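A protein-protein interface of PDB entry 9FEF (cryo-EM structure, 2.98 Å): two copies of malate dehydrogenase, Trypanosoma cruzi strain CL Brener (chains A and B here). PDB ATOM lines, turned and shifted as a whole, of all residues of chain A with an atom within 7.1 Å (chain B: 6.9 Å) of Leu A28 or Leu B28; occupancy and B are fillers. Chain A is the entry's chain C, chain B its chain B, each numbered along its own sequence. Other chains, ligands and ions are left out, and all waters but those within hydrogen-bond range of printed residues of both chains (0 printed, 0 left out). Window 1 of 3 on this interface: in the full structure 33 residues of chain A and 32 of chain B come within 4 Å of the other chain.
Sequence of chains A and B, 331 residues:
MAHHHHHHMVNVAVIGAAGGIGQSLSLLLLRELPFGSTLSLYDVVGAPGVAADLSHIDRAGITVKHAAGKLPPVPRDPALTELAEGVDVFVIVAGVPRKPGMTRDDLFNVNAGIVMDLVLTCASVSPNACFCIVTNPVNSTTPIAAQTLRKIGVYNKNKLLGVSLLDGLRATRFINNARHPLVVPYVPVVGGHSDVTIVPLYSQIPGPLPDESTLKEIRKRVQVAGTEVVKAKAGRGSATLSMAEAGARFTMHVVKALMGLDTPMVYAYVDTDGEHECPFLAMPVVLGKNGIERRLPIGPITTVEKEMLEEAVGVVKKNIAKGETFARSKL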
ATOM      1  N   GLY A  22     -22.426   4.902   2.674  1.00  0.00           N
ATOM      2  CA  GLY A  22     -23.217   3.826   3.241  1.00  0.00           C
ATOM      3  C   GLY A  22     -23.017   2.485   2.572  1.00  0.00           C
ATOM      4  O   GLY A  22     -23.142   1.452   3.236  1.00  0.00           O
ATOM      5  N   GLN A  23     -22.714   2.472   1.274  1.00  0.00           N
ATOM      6  CA  GLN A  23     -22.530   1.209   0.565  1.00  0.00           C
ATOM      7  C   GLN A  23     -21.297   0.464   1.067  1.00  0.00           C
ATOM      8  O   GLN A  23     -21.373  -0.722   1.411  1.00  0.00           O
ATOM      9  CB  GLN A  23     -22.431   1.467  -0.937  1.00  0.00           C
ATOM     10  CG  GLN A  23     -23.736   1.267  -1.680  1.00  0.00           C
ATOM     11  CD  GLN A  23     -23.552   1.235  -3.181  1.00  0.00           C
ATOM     12  OE1 GLN A  23     -22.664   0.558  -3.693  1.00  0.00           O
ATOM     13  NE2 GLN A  23     -24.397   1.966  -3.895  1.00  0.00           N
ATOM     14  N   SER A  24     -20.152   1.146   1.126  1.00  0.00           N
ATOM     15  CA  SER A  24     -18.937   0.505   1.618  1.00  0.00           C
ATOM     16  C   SER A  24     -19.017   0.216   3.111  1.00  0.00           C
ATOM     17  O   SER A  24     -18.469  -0.790   3.576  1.00  0.00           O
ATOM     18  CB  SER A  24     -17.719   1.374   1.308  1.00  0.00           C
ATOM     19  OG  SER A  24     -17.510   1.480  -0.088  1.00  0.00           O
ATOM     20  N   LEU A  25     -19.683   1.082   3.875  1.00  0.00           N
ATOM     21  CA  LEU A  25     -19.886   0.814   5.293  1.00  0.00           C
ATOM     22  C   LEU A  25     -20.718  -0.445   5.496  1.00  0.00           C
ATOM     23  O   LEU A  25     -20.423  -1.261   6.376  1.00  0.00           O
ATOM     24  CB  LEU A  25     -20.558   2.015   5.958  1.00  0.00           C
ATOM     25  CG  LEU A  25     -20.431   2.177   7.471  1.00  0.00           C
ATOM     26  CD1 LEU A  25     -20.150   3.625   7.813  1.00  0.00           C
ATOM     27  CD2 LEU A  25     -21.688   1.705   8.170  1.00  0.00           C
ATOM     28  N   SER A  26     -21.768  -0.616   4.689  1.00  0.00           N
ATOM     29  CA  SER A  26     -22.599  -1.810   4.777  1.00  0.00           C
ATOM     30  C   SER A  26     -21.833  -3.054   4.348  1.00  0.00           C
ATOM     31  O   SER A  26     -21.973  -4.118   4.960  1.00  0.00           O
ATOM     32  CB  SER A  26     -23.851  -1.632   3.923  1.00  0.00           C
ATOM     33  OG  SER A  26     -24.876  -0.988   4.654  1.00  0.00           O
ATOM     34  N   LEU A  27     -21.030  -2.944   3.287  1.00  0.00           N
ATOM     35  CA  LEU A  27     -20.247  -4.090   2.837  1.00  0.00           C
ATOM     36  C   LEU A  27     -19.219  -4.506   3.882  1.00  0.00           C
ATOM     37  O   LEU A  27     -19.000  -5.701   4.104  1.00  0.00           O
ATOM     38  CB  LEU A  27     -19.567  -3.771   1.507  1.00  0.00           C
ATOM     39  CG  LEU A  27     -18.357  -4.626   1.125  1.00  0.00           C
ATOM     40  CD1 LEU A  27     -18.792  -6.017   0.701  1.00  0.00           C
ATOM     41  CD2 LEU A  27     -17.567  -3.957   0.017  1.00  0.00           C
ATOM     42  N   LEU A  28     -18.573  -3.534   4.532  1.00  0.00           N
ATOM     43  CA  LEU A  28     -17.578  -3.857   5.549  1.00  0.00           C
ATOM     44  C   LEU A  28     -18.215  -4.449   6.797  1.00  0.00           C
ATOM     45  O   LEU A  28     -17.618  -5.318   7.442  1.00  0.00           O
ATOM     46  CB  LEU A  28     -16.775  -2.609   5.911  1.00  0.00           C
ATOM     47  CG  LEU A  28     -15.723  -2.165   4.897  1.00  0.00           C
ATOM     48  CD1 LEU A  28     -14.972  -0.957   5.415  1.00  0.00           C
ATOM     49  CD2 LEU A  28     -14.767  -3.298   4.586  1.00  0.00           C
ATOM     50  N   LEU A  29     -19.413  -3.987   7.162  1.00  0.00           N
ATOM     51  CA  LEU A  29     -20.080  -4.507   8.352  1.00  0.00           C
ATOM     52  C   LEU A  29     -20.469  -5.970   8.181  1.00  0.00           C
ATOM     53  O   LEU A  29     -20.321  -6.768   9.113  1.00  0.00           O
ATOM     54  CB  LEU A  29     -21.310  -3.663   8.676  1.00  0.00           C
ATOM     55  CG  LEU A  29     -21.074  -2.389   9.486  1.00  0.00           C
ATOM     56  CD1 LEU A  29     -22.393  -1.717   9.808  1.00  0.00           C
ATOM     57  CD2 LEU A  29     -20.311  -2.702  10.755  1.00  0.00           C
ATOM     58  N   LEU A  30     -20.961  -6.341   6.997  1.00  0.00           N
ATOM     59  CA  LEU A  30     -21.414  -7.711   6.773  1.00  0.00           C
ATOM     60  C   LEU A  30     -20.292  -8.720   6.971  1.00  0.00           C
ATOM     61  O   LEU A  30     -20.538  -9.835   7.444  1.00  0.00           O
ATOM     62  CB  LEU A  30     -22.003  -7.842   5.368  1.00  0.00           C
ATOM     63  CG  LEU A  30     -22.570  -9.208   4.985  1.00  0.00           C
ATOM     64  CD1 LEU A  30     -24.086  -9.179   4.983  1.00  0.00           C
ATOM     65  CD2 LEU A  30     -22.038  -9.635   3.631  1.00  0.00           C
ATOM     66  N   ARG A  31     -19.058  -8.351   6.635  1.00  0.00           N
ATOM     67  CA  ARG A  31     -17.929  -9.257   6.792  1.00  0.00           C
ATOM     68  C   ARG A  31     -17.396  -9.313   8.216  1.00  0.00           C
ATOM     69  O   ARG A  31     -16.518 -10.137   8.493  1.00  0.00           O
ATOM     70  CB  ARG A  31     -16.795  -8.855   5.851  1.00  0.00           C
ATOM     71  CG  ARG A  31     -17.234  -8.562   4.433  1.00  0.00           C
ATOM     72  CD  ARG A  31     -16.244  -7.648   3.738  1.00  0.00           C
ATOM     73  NE  ARG A  31     -15.119  -8.386   3.179  1.00  0.00           N
ATOM     74  CZ  ARG A  31     -13.946  -8.533   3.781  1.00  0.00           C
ATOM     75  NH1 ARG A  31     -13.705  -7.999   4.966  1.00  0.00           N
ATOM     76  NH2 ARG A  31     -12.991  -9.233   3.176  1.00  0.00           N
ATOM     77  N   GLU A  32     -17.890  -8.465   9.121  1.00  0.00           N
ATOM     78  CA  GLU A  32     -17.366  -8.412  10.478  1.00  0.00           C
ATOM     79  C   GLU A  32     -18.417  -8.540  11.571  1.00  0.00           C
ATOM     80  O   GLU A  32     -18.038  -8.712  12.735  1.00  0.00           O
ATOM     81  CB  GLU A  32     -16.584  -7.109  10.701  1.00  0.00           C
ATOM     82  CG  GLU A  32     -15.345  -6.981   9.833  1.00  0.00           C
ATOM     83  CD  GLU A  32     -14.063  -7.101  10.630  1.00  0.00           C
ATOM     84  OE1 GLU A  32     -12.984  -6.813  10.072  1.00  0.00           O
ATOM     85  OE2 GLU A  32     -14.133  -7.486  11.817  1.00  0.00           O
ATOM     86  N   LEU A  33     -19.705  -8.464  11.252  1.00  0.00           N
ATOM     87  CA  LEU A  33     -20.724  -8.650  12.273  1.00  0.00           C
ATOM     88  C   LEU A  33     -20.610 -10.059  12.855  1.00  0.00           C
ATOM     89  O   LEU A  33     -20.295 -11.005  12.125  1.00  0.00           O
ATOM     90  CB  LEU A  33     -22.124  -8.443  11.690  1.00  0.00           C
ATOM     91  CG  LEU A  33     -22.910  -7.145  11.926  1.00  0.00           C
ATOM     92  CD1 LEU A  33     -23.327  -7.004  13.378  1.00  0.00           C
ATOM     93  CD2 LEU A  33     -22.155  -5.922  11.472  1.00  0.00           C
ATOM     94  N   LEU A  54     -25.740  -7.826  -1.155  1.00  0.00           N
ATOM     95  CA  LEU A  54     -25.036  -8.458  -0.050  1.00  0.00           C
ATOM     96  C   LEU A  54     -25.700  -9.750   0.393  1.00  0.00           C
ATOM     97  O   LEU A  54     -25.103 -10.500   1.174  1.00  0.00           O
ATOM     98  CB  LEU A  54     -24.949  -7.495   1.134  1.00  0.00           C
ATOM     99  CG  LEU A  54     -24.396  -6.102   0.845  1.00  0.00           C
ATOM    100  CD1 LEU A  54     -24.926  -5.110   1.860  1.00  0.00           C
ATOM    101  CD2 LEU A  54     -22.881  -6.122   0.855  1.00  0.00           C
ATOM    102  N   LEU A 241     -13.997   6.591   1.088  1.00  0.00           N
ATOM    103  CA  LEU A 241     -13.516   5.251   1.405  1.00  0.00           C
ATOM    104  C   LEU A 241     -12.940   5.143   2.808  1.00  0.00           C
ATOM    105  O   LEU A 241     -13.124   4.117   3.469  1.00  0.00           O
ATOM    106  CB  LEU A 241     -12.461   4.813   0.385  1.00  0.00           C
ATOM    107  CG  LEU A 241     -12.979   4.303  -0.961  1.00  0.00           C
ATOM    108  CD1 LEU A 241     -11.844   3.739  -1.795  1.00  0.00           C
ATOM    109  CD2 LEU A 241     -14.062   3.260  -0.759  1.00  0.00           C
ATOM    110  N   ALA A 244     -15.908   5.428   5.411  1.00  0.00           N
ATOM    111  CA  ALA A 244     -16.586   4.148   5.579  1.00  0.00           C
ATOM    112  C   ALA A 244     -15.811   3.230   6.512  1.00  0.00           C
ATOM    113  O   ALA A 244     -16.400   2.567   7.371  1.00  0.00           O
ATOM    114  CB  ALA A 244     -16.788   3.483   4.219  1.00  0.00           C
ATOM    115  N   GLU A 245     -14.485   3.180   6.359  1.00  0.00           N
ATOM    116  CA  GLU A 245     -13.668   2.339   7.228  1.00  0.00           C
ATOM    117  C   GLU A 245     -13.733   2.804   8.679  1.00  0.00           C
ATOM    118  O   GLU A 245     -13.866   1.984   9.597  1.00  0.00           O
ATOM    119  CB  GLU A 245     -12.224   2.328   6.731  1.00  0.00           C
ATOM    120  CG  GLU A 245     -11.221   1.828   7.748  1.00  0.00           C
ATOM    121  CD  GLU A 245     -11.092   0.320   7.741  1.00  0.00           C
ATOM    122  OE1 GLU A 245     -11.965  -0.354   8.326  1.00  0.00           O
ATOM    123  OE2 GLU A 245     -10.118  -0.193   7.152  1.00  0.00           O
ATOM    124  N   ALA A 246     -13.648   4.117   8.907  1.00  0.00           N
ATOM    125  CA  ALA A 246     -13.733   4.635  10.269  1.00  0.00           C
ATOM    126  C   ALA A 246     -15.095   4.344  10.889  1.00  0.00           C
ATOM    127  O   ALA A 246     -15.182   3.926  12.053  1.00  0.00           O
ATOM    128  CB  ALA A 246     -13.450   6.135  10.276  1.00  0.00           C
ATOM    129  N   ALA A 248     -17.192   1.914  10.079  1.00  0.00           N
ATOM    130  CA  ALA A 248     -17.302   0.480  10.320  1.00  0.00           C
ATOM    131  C   ALA A 248     -16.526   0.066  11.562  1.00  0.00           C
ATOM    132  O   ALA A 248     -17.015  -0.732  12.368  1.00  0.00           O
ATOM    133  CB  ALA A 248     -16.813  -0.297   9.099  1.00  0.00           C
ATOM    134  N   ARG A 249     -15.314   0.600  11.737  1.00  0.00           N
ATOM    135  CA  ARG A 249     -14.520   0.250  12.911  1.00  0.00           C
ATOM    136  C   ARG A 249     -15.183   0.728  14.199  1.00  0.00           C
ATOM    137  O   ARG A 249     -15.226  -0.010  15.194  1.00  0.00           O
ATOM    138  CB  ARG A 249     -13.114   0.830  12.775  1.00  0.00           C
ATOM    139  CG  ARG A 249     -12.104   0.235  13.737  1.00  0.00           C
ATOM    140  CD  ARG A 249     -10.760   0.930  13.620  1.00  0.00           C
ATOM    141  NE  ARG A 249     -10.235   0.883  12.261  1.00  0.00           N
ATOM    142  CZ  ARG A 249      -8.953   0.741  11.958  1.00  0.00           C
ATOM    143  NH1 ARG A 249      -8.029   0.634  12.898  1.00  0.00           N
ATOM    144  NH2 ARG A 249      -8.587   0.708  10.680  1.00  0.00           N
ATOM    145  N   MET A 252     -18.131  -1.476  14.928  1.00  0.00           N
ATOM    146  CA  MET A 252     -17.664  -2.745  15.476  1.00  0.00           C
ATOM    147  C   MET A 252     -17.305  -2.617  16.948  1.00  0.00           C
ATOM    148  O   MET A 252     -17.639  -3.495  17.749  1.00  0.00           O
ATOM    149  CB  MET A 252     -16.472  -3.260  14.672  1.00  0.00           C
ATOM    150  CG  MET A 252     -16.807  -4.307  13.612  1.00  0.00           C
ATOM    151  SD  MET A 252     -17.977  -5.573  14.153  1.00  0.00           S
ATOM    152  CE  MET A 252     -19.534  -4.908  13.574  1.00  0.00           C
ATOM    153  N   GLY B  22     -13.948  -1.441  -8.682  1.00  0.00           N
ATOM    154  CA  GLY B  22     -12.546  -1.251  -8.348  1.00  0.00           C
ATOM    155  C   GLY B  22     -12.329  -0.552  -7.022  1.00  0.00           C
ATOM    156  O   GLY B  22     -11.391  -0.875  -6.291  1.00  0.00           O
ATOM    157  N   GLN B  23     -13.183   0.420  -6.694  1.00  0.00           N
ATOM    158  CA  GLN B  23     -13.036   1.138  -5.433  1.00  0.00           C
ATOM    159  C   GLN B  23     -13.205   0.200  -4.243  1.00  0.00           C
ATOM    160  O   GLN B  23     -12.367   0.170  -3.332  1.00  0.00           O
ATOM    161  CB  GLN B  23     -14.048   2.281  -5.366  1.00  0.00           C
ATOM    162  CG  GLN B  23     -13.626   3.527  -6.119  1.00  0.00           C
ATOM    163  CD  GLN B  23     -14.498   4.722  -5.798  1.00  0.00           C
ATOM    164  OE1 GLN B  23     -15.398   4.640  -4.964  1.00  0.00           O
ATOM    165  NE2 GLN B  23     -14.239   5.840  -6.462  1.00  0.00           N
ATOM    166  N   SER B  24     -14.286  -0.582  -4.240  1.00  0.00           N
ATOM    167  CA  SER B  24     -14.517  -1.527  -3.154  1.00  0.00           C
ATOM    168  C   SER B  24     -13.450  -2.614  -3.130  1.00  0.00           C
ATOM    169  O   SER B  24     -13.026  -3.048  -2.052  1.00  0.00           O
ATOM    170  CB  SER B  24     -15.910  -2.142  -3.281  1.00  0.00           C
ATOM    171  OG  SER B  24     -16.912  -1.143  -3.274  1.00  0.00           O
ATOM    172  N   LEU B  25     -13.003  -3.066  -4.303  1.00  0.00           N
ATOM    173  CA  LEU B  25     -11.961  -4.086  -4.344  1.00  0.00           C
ATOM    174  C   LEU B  25     -10.662  -3.565  -3.744  1.00  0.00           C
ATOM    175  O   LEU B  25      -9.994  -4.275  -2.985  1.00  0.00           O
ATOM    176  CB  LEU B  25     -11.745  -4.551  -5.785  1.00  0.00           C
ATOM    177  CG  LEU B  25     -10.882  -5.790  -6.022  1.00  0.00           C
ATOM    178  CD1 LEU B  25     -11.559  -6.707  -7.020  1.00  0.00           C
ATOM    179  CD2 LEU B  25      -9.501  -5.409  -6.507  1.00  0.00           C
ATOM    180  N   SER B  26     -10.290  -2.324  -4.066  1.00  0.00           N
ATOM    181  CA  SER B  26      -9.087  -1.728  -3.495  1.00  0.00           C
ATOM    182  C   SER B  26      -9.225  -1.531  -1.992  1.00  0.00           C
ATOM    183  O   SER B  26      -8.273  -1.771  -1.239  1.00  0.00           O
ATOM    184  CB  SER B  26      -8.786  -0.398  -4.182  1.00  0.00           C
ATOM    185  OG  SER B  26      -8.954  -0.498  -5.583  1.00  0.00           O
ATOM    186  N   LEU B  27     -10.400  -1.090  -1.536  1.00  0.00           N
ATOM    187  CA  LEU B  27     -10.616  -0.933  -0.102  1.00  0.00           C
ATOM    188  C   LEU B  27     -10.473  -2.263   0.624  1.00  0.00           C
ATOM    189  O   LEU B  27      -9.865  -2.330   1.697  1.00  0.00           O
ATOM    190  CB  LEU B  27     -11.992  -0.322   0.162  1.00  0.00           C
ATOM    191  CG  LEU B  27     -12.449  -0.268   1.620  1.00  0.00           C
ATOM    192  CD1 LEU B  27     -11.462   0.515   2.468  1.00  0.00           C
ATOM    193  CD2 LEU B  27     -13.841   0.331   1.726  1.00  0.00           C
ATOM    194  N   LEU B  28     -11.027  -3.334   0.053  1.00  0.00           N
ATOM    195  CA  LEU B  28     -10.910  -4.648   0.678  1.00  0.00           C
ATOM    196  C   LEU B  28      -9.474  -5.158   0.641  1.00  0.00           C
ATOM    197  O   LEU B  28      -9.006  -5.772   1.604  1.00  0.00           O
ATOM    198  CB  LEU B  28     -11.847  -5.639  -0.011  1.00  0.00           C
ATOM    199  CG  LEU B  28     -13.342  -5.433   0.230  1.00  0.00           C
ATOM    200  CD1 LEU B  28     -14.136  -6.576  -0.364  1.00  0.00           C
ATOM    201  CD2 LEU B  28     -13.626  -5.295   1.710  1.00  0.00           C
ATOM    202  N   LEU B  29      -8.761  -4.919  -0.462  1.00  0.00           N
ATOM    203  CA  LEU B  29      -7.396  -5.420  -0.587  1.00  0.00           C
ATOM    204  C   LEU B  29      -6.428  -4.667   0.316  1.00  0.00           C
ATOM    205  O   LEU B  29      -5.402  -5.224   0.717  1.00  0.00           O
ATOM    206  CB  LEU B  29      -6.938  -5.329  -2.041  1.00  0.00           C
ATOM    207  CG  LEU B  29      -7.111  -6.581  -2.903  1.00  0.00           C
ATOM    208  CD1 LEU B  29      -6.620  -6.318  -4.312  1.00  0.00           C
ATOM    209  CD2 LEU B  29      -6.382  -7.762  -2.292  1.00  0.00           C
ATOM    210  N   LEU B  30      -6.724  -3.404   0.634  1.00  0.00           N
ATOM    211  CA  LEU B  30      -5.841  -2.645   1.514  1.00  0.00           C
ATOM    212  C   LEU B  30      -5.793  -3.247   2.913  1.00  0.00           C
ATOM    213  O   LEU B  30      -4.733  -3.277   3.547  1.00  0.00           O
ATOM    214  CB  LEU B  30      -6.289  -1.185   1.577  1.00  0.00           C
ATOM    215  CG  LEU B  30      -5.389  -0.233   2.366  1.00  0.00           C
ATOM    216  CD1 LEU B  30      -4.143   0.115   1.574  1.00  0.00           C
ATOM    217  CD2 LEU B  30      -6.148   1.020   2.743  1.00  0.00           C
ATOM    218  N   ARG B  31      -6.930  -3.730   3.414  1.00  0.00           N
ATOM    219  CA  ARG B  31      -6.999  -4.245   4.775  1.00  0.00           C
ATOM    220  C   ARG B  31      -6.522  -5.686   4.910  1.00  0.00           C
ATOM    221  O   ARG B  31      -6.320  -6.142   6.039  1.00  0.00           O
ATOM    222  CB  ARG B  31      -8.430  -4.142   5.305  1.00  0.00           C
ATOM    223  CG  ARG B  31      -9.208  -2.958   4.777  1.00  0.00           C
ATOM    224  CD  ARG B  31     -10.698  -3.250   4.750  1.00  0.00           C
ATOM    225  NE  ARG B  31     -11.322  -3.036   6.049  1.00  0.00           N
ATOM    226  CZ  ARG B  31     -11.664  -4.007   6.885  1.00  0.00           C
ATOM    227  NH1 ARG B  31     -11.456  -5.278   6.588  1.00  0.00           N
ATOM    228  NH2 ARG B  31     -12.229  -3.695   8.047  1.00  0.00           N
ATOM    229  N   GLU B  32      -6.340  -6.414   3.806  1.00  0.00           N
ATOM    230  CA  GLU B  32      -5.987  -7.825   3.879  1.00  0.00           C
ATOM    231  C   GLU B  32      -4.599  -8.155   3.352  1.00  0.00           C
ATOM    232  O   GLU B  32      -4.104  -9.252   3.627  1.00  0.00           O
ATOM    233  CB  GLU B  32      -7.010  -8.676   3.116  1.00  0.00           C
ATOM    234  CG  GLU B  32      -8.457  -8.293   3.359  1.00  0.00           C
ATOM    235  CD  GLU B  32      -8.987  -8.823   4.674  1.00  0.00           C
ATOM    236  OE1 GLU B  32      -8.394  -9.782   5.211  1.00  0.00           O
ATOM    237  OE2 GLU B  32      -9.999  -8.283   5.167  1.00  0.00           O
ATOM    238  N   LEU B  33      -3.965  -7.257   2.604  1.00  0.00           N
ATOM    239  CA  LEU B  33      -2.655  -7.554   2.053  1.00  0.00           C
ATOM    240  C   LEU B  33      -1.629  -7.711   3.175  1.00  0.00           C
ATOM    241  O   LEU B  33      -1.729  -7.058   4.215  1.00  0.00           O
ATOM    242  CB  LEU B  33      -2.214  -6.451   1.094  1.00  0.00           C
ATOM    243  CG  LEU B  33      -2.642  -6.587  -0.368  1.00  0.00           C
ATOM    244  CD1 LEU B  33      -2.498  -5.260  -1.091  1.00  0.00           C
ATOM    245  CD2 LEU B  33      -1.841  -7.664  -1.068  1.00  0.00           C
ATOM    246  N   LEU B  54      -7.121   6.175   0.092  1.00  0.00           N
ATOM    247  CA  LEU B  54      -6.658   4.994   0.806  1.00  0.00           C
ATOM    248  C   LEU B  54      -5.335   5.215   1.524  1.00  0.00           C
ATOM    249  O   LEU B  54      -4.934   4.362   2.322  1.00  0.00           O
ATOM    250  CB  LEU B  54      -6.520   3.810  -0.158  1.00  0.00           C
ATOM    251  CG  LEU B  54      -7.768   3.391  -0.935  1.00  0.00           C
ATOM    252  CD1 LEU B  54      -7.388   2.454  -2.062  1.00  0.00           C
ATOM    253  CD2 LEU B  54      -8.774   2.735  -0.013  1.00  0.00           C
ATOM    254  N   LEU B 241     -20.743  -4.913  -5.193  1.00  0.00           N
ATOM    255  CA  LEU B 241     -20.202  -5.341  -3.909  1.00  0.00           C
ATOM    256  C   LEU B 241     -19.848  -6.823  -3.900  1.00  0.00           C
ATOM    257  O   LEU B 241     -18.768  -7.198  -3.426  1.00  0.00           O
ATOM    258  CB  LEU B 241     -21.202  -5.029  -2.797  1.00  0.00           C
ATOM    259  CG  LEU B 241     -21.591  -3.556  -2.648  1.00  0.00           C
ATOM    260  CD1 LEU B 241     -22.723  -3.389  -1.652  1.00  0.00           C
ATOM    261  CD2 LEU B 241     -20.391  -2.722  -2.236  1.00  0.00           C
ATOM    262  N   ALA B 244     -16.809  -7.390  -6.129  1.00  0.00           N
ATOM    263  CA  ALA B 244     -15.619  -6.892  -5.448  1.00  0.00           C
ATOM    264  C   ALA B 244     -15.159  -7.856  -4.365  1.00  0.00           C
ATOM    265  O   ALA B 244     -13.959  -8.125  -4.234  1.00  0.00           O
ATOM    266  CB  ALA B 244     -15.894  -5.512  -4.855  1.00  0.00           C
ATOM    267  N   GLU B 245     -16.098  -8.392  -3.582  1.00  0.00           N
ATOM    268  CA  GLU B 245     -15.740  -9.367  -2.557  1.00  0.00           C
ATOM    269  C   GLU B 245     -15.111 -10.613  -3.170  1.00  0.00           C
ATOM    270  O   GLU B 245     -14.083 -11.105  -2.683  1.00  0.00           O
ATOM    271  CB  GLU B 245     -16.974  -9.739  -1.738  1.00  0.00           C
ATOM    272  CG  GLU B 245     -16.753 -10.888  -0.776  1.00  0.00           C
ATOM    273  CD  GLU B 245     -16.672 -10.433   0.664  1.00  0.00           C
ATOM    274  OE1 GLU B 245     -16.848  -9.224   0.915  1.00  0.00           O
ATOM    275  OE2 GLU B 245     -16.432 -11.285   1.546  1.00  0.00           O
ATOM    276  N   ALA B 246     -15.710 -11.135  -4.244  1.00  0.00           N
ATOM    277  CA  ALA B 246     -15.170 -12.330  -4.886  1.00  0.00           C
ATOM    278  C   ALA B 246     -13.779 -12.078  -5.459  1.00  0.00           C
ATOM    279  O   ALA B 246     -12.873 -12.909  -5.303  1.00  0.00           O
ATOM    280  CB  ALA B 246     -16.122 -12.809  -5.979  1.00  0.00           C
ATOM    281  N   ALA B 248     -11.590  -9.793  -4.501  1.00  0.00           N
ATOM    282  CA  ALA B 248     -10.650  -9.639  -3.398  1.00  0.00           C
ATOM    283  C   ALA B 248     -10.269 -10.987  -2.804  1.00  0.00           C
ATOM    284  O   ALA B 248      -9.095 -11.228  -2.501  1.00  0.00           O
ATOM    285  CB  ALA B 248     -11.244  -8.726  -2.326  1.00  0.00           C
ATOM    286  N   ARG B 249     -11.245 -11.886  -2.639  1.00  0.00           N
ATOM    287  CA  ARG B 249     -10.945 -13.210  -2.099  1.00  0.00           C
ATOM    288  C   ARG B 249     -10.006 -13.984  -3.017  1.00  0.00           C
ATOM    289  O   ARG B 249      -9.028 -14.590  -2.560  1.00  0.00           O
ATOM    290  CB  ARG B 249     -12.241 -13.990  -1.876  1.00  0.00           C
ATOM    291  CG  ARG B 249     -13.050 -13.519  -0.683  1.00  0.00           C
ATOM    292  CD  ARG B 249     -13.133 -14.593   0.386  1.00  0.00           C
ATOM    293  NE  ARG B 249     -14.169 -15.579   0.105  1.00  0.00           N
ATOM    294  CZ  ARG B 249     -15.403 -15.524   0.585  1.00  0.00           C
ATOM    295  NH1 ARG B 249     -15.800 -14.528   1.357  1.00  0.00           N
ATOM    296  NH2 ARG B 249     -16.261 -16.494   0.283  1.00  0.00           N
ATOM    297  N   MET B 252      -6.509 -12.472  -2.915  1.00  0.00           N
ATOM    298  CA  MET B 252      -5.834 -12.860  -1.682  1.00  0.00           C
ATOM    299  C   MET B 252      -5.335 -14.297  -1.758  1.00  0.00           C
ATOM    300  O   MET B 252      -4.223 -14.597  -1.309  1.00  0.00           O
ATOM    301  CB  MET B 252      -6.770 -12.675  -0.488  1.00  0.00           C
ATOM    302  CG  MET B 252      -6.653 -11.319   0.192  1.00  0.00           C
ATOM    303  SD  MET B 252      -4.968 -10.685   0.225  1.00  0.00           S
ATOM    304  CE  MET B 252      -4.216 -11.779   1.426  1.00  0.00           C
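OE1 of Glu A32 is in salt-bridge range of NH2 of Arg B31, at 3.8 Å. The side-chain carboxylate of Glu A245 lies within salt-bridge range of the guanidinium group of Arg B31, 3.3 Å away. NH2 of Arg A31 is in salt-bridge range of OE2 of Glu B32, 3.7 Å away. OE1 of Glu B245 lies within salt-bridge range of NE of Arg A31 (3.0 Å).
The guanidinium group (NH1) of Arg B31 lies within salt-bridge range of the side-chain carboxylate (OE2) of Glu B32 (3.6 Å). The side-chain carboxylate (OE2) of Glu B245 is in salt-bridge range of the guanidinium group (NH1) of Arg B249. The guanidinium group (NH2) of Arg A249 lies within salt-bridge range of the side-chain carboxylate (OE2) of Glu A245.
Among the printed residues, merely in contact across the chains: Leu A27 with Leu B241 (3.8 Å), Leu A27 with Glu B245 (3.8 Å), Leu A28 with Leu B28 (3.7 Å), Leu A28 with Arg B31 (3.8 Å), Arg A31 with Leu B28 (3.7 Å), Arg A31 with Arg B31 (3.9 Å), Leu A54 with Leu B241 (3.7 Å), Leu A241 with Gln B23 (3.9 Å), Leu A241 with Leu B27 (3.8 Å) and Leu A241 with Leu B54 (3.7 Å).
Leu A28 touches just these residues of chain B: Leu B28 and Arg B31. Of chain A, only Leu A28 (3.7 Å) and Arg A31 (3.7 Å) come within 4 Å of Leu B28. Of the printed residues of chain B, Leu A27 touches Leu B241 (3.8 Å) and Glu B245 (3.8 Å). Printed residues of chain B within 4 Å of Leu A54: Leu B241. Of the printed residues of chain B, Leu A241 touches Gln B23 (3.9 Å), Leu B27 (3.8 Å) and Leu B54 (3.7 Å). Ser B24 touches none of the printed residues of chain A. Ala A244 touches none of the printed residues of chain B. The nearest residue of chain B that does not touch Leu A28 is Leu B27 (4.1 Å). The nearest residue of chain A that does not touch Leu B28 is Leu A27 (4.3 Å). The nearest printed residue of chain A that does not touch Leu B54 is Glu A245 (7.6 Å).
Printed residues of chain B that touch a printed residue of chain A: Gln B23, Leu B27, Leu B28, Arg B31, Glu B32, Leu B54, Leu B241 and Glu B245. Hydrophobic or aromatic side chains of chain B within 4 Å of the printed part of chain A: Leu B27, Leu B28, Leu B54 and Leu B241. Of the 20 printed residues of chain A, 7 touch a printed residue of chain B. Printed residues of chain A that touch a printed residue of chain B: Leu A27, Leu A28, Arg A31, Glu A32, Leu A54, Leu A241 and Glu A245. Hydrophobic or aromatic side chains of chain A that line the printed part of chain B: Leu A27, Leu A28, Leu A54 and Leu A241.
Leu A27 touches Glu B245, but with the chains exchanged Glu A245 does not touch Leu B27 (4.7 Å). Leu A28 touches Arg B31, and with the chains exchanged Arg A31 touches Leu B28. Of the 14 pairs that touch across the chains among the printed residues, 12 have their exchanged pair printed and touching as well.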
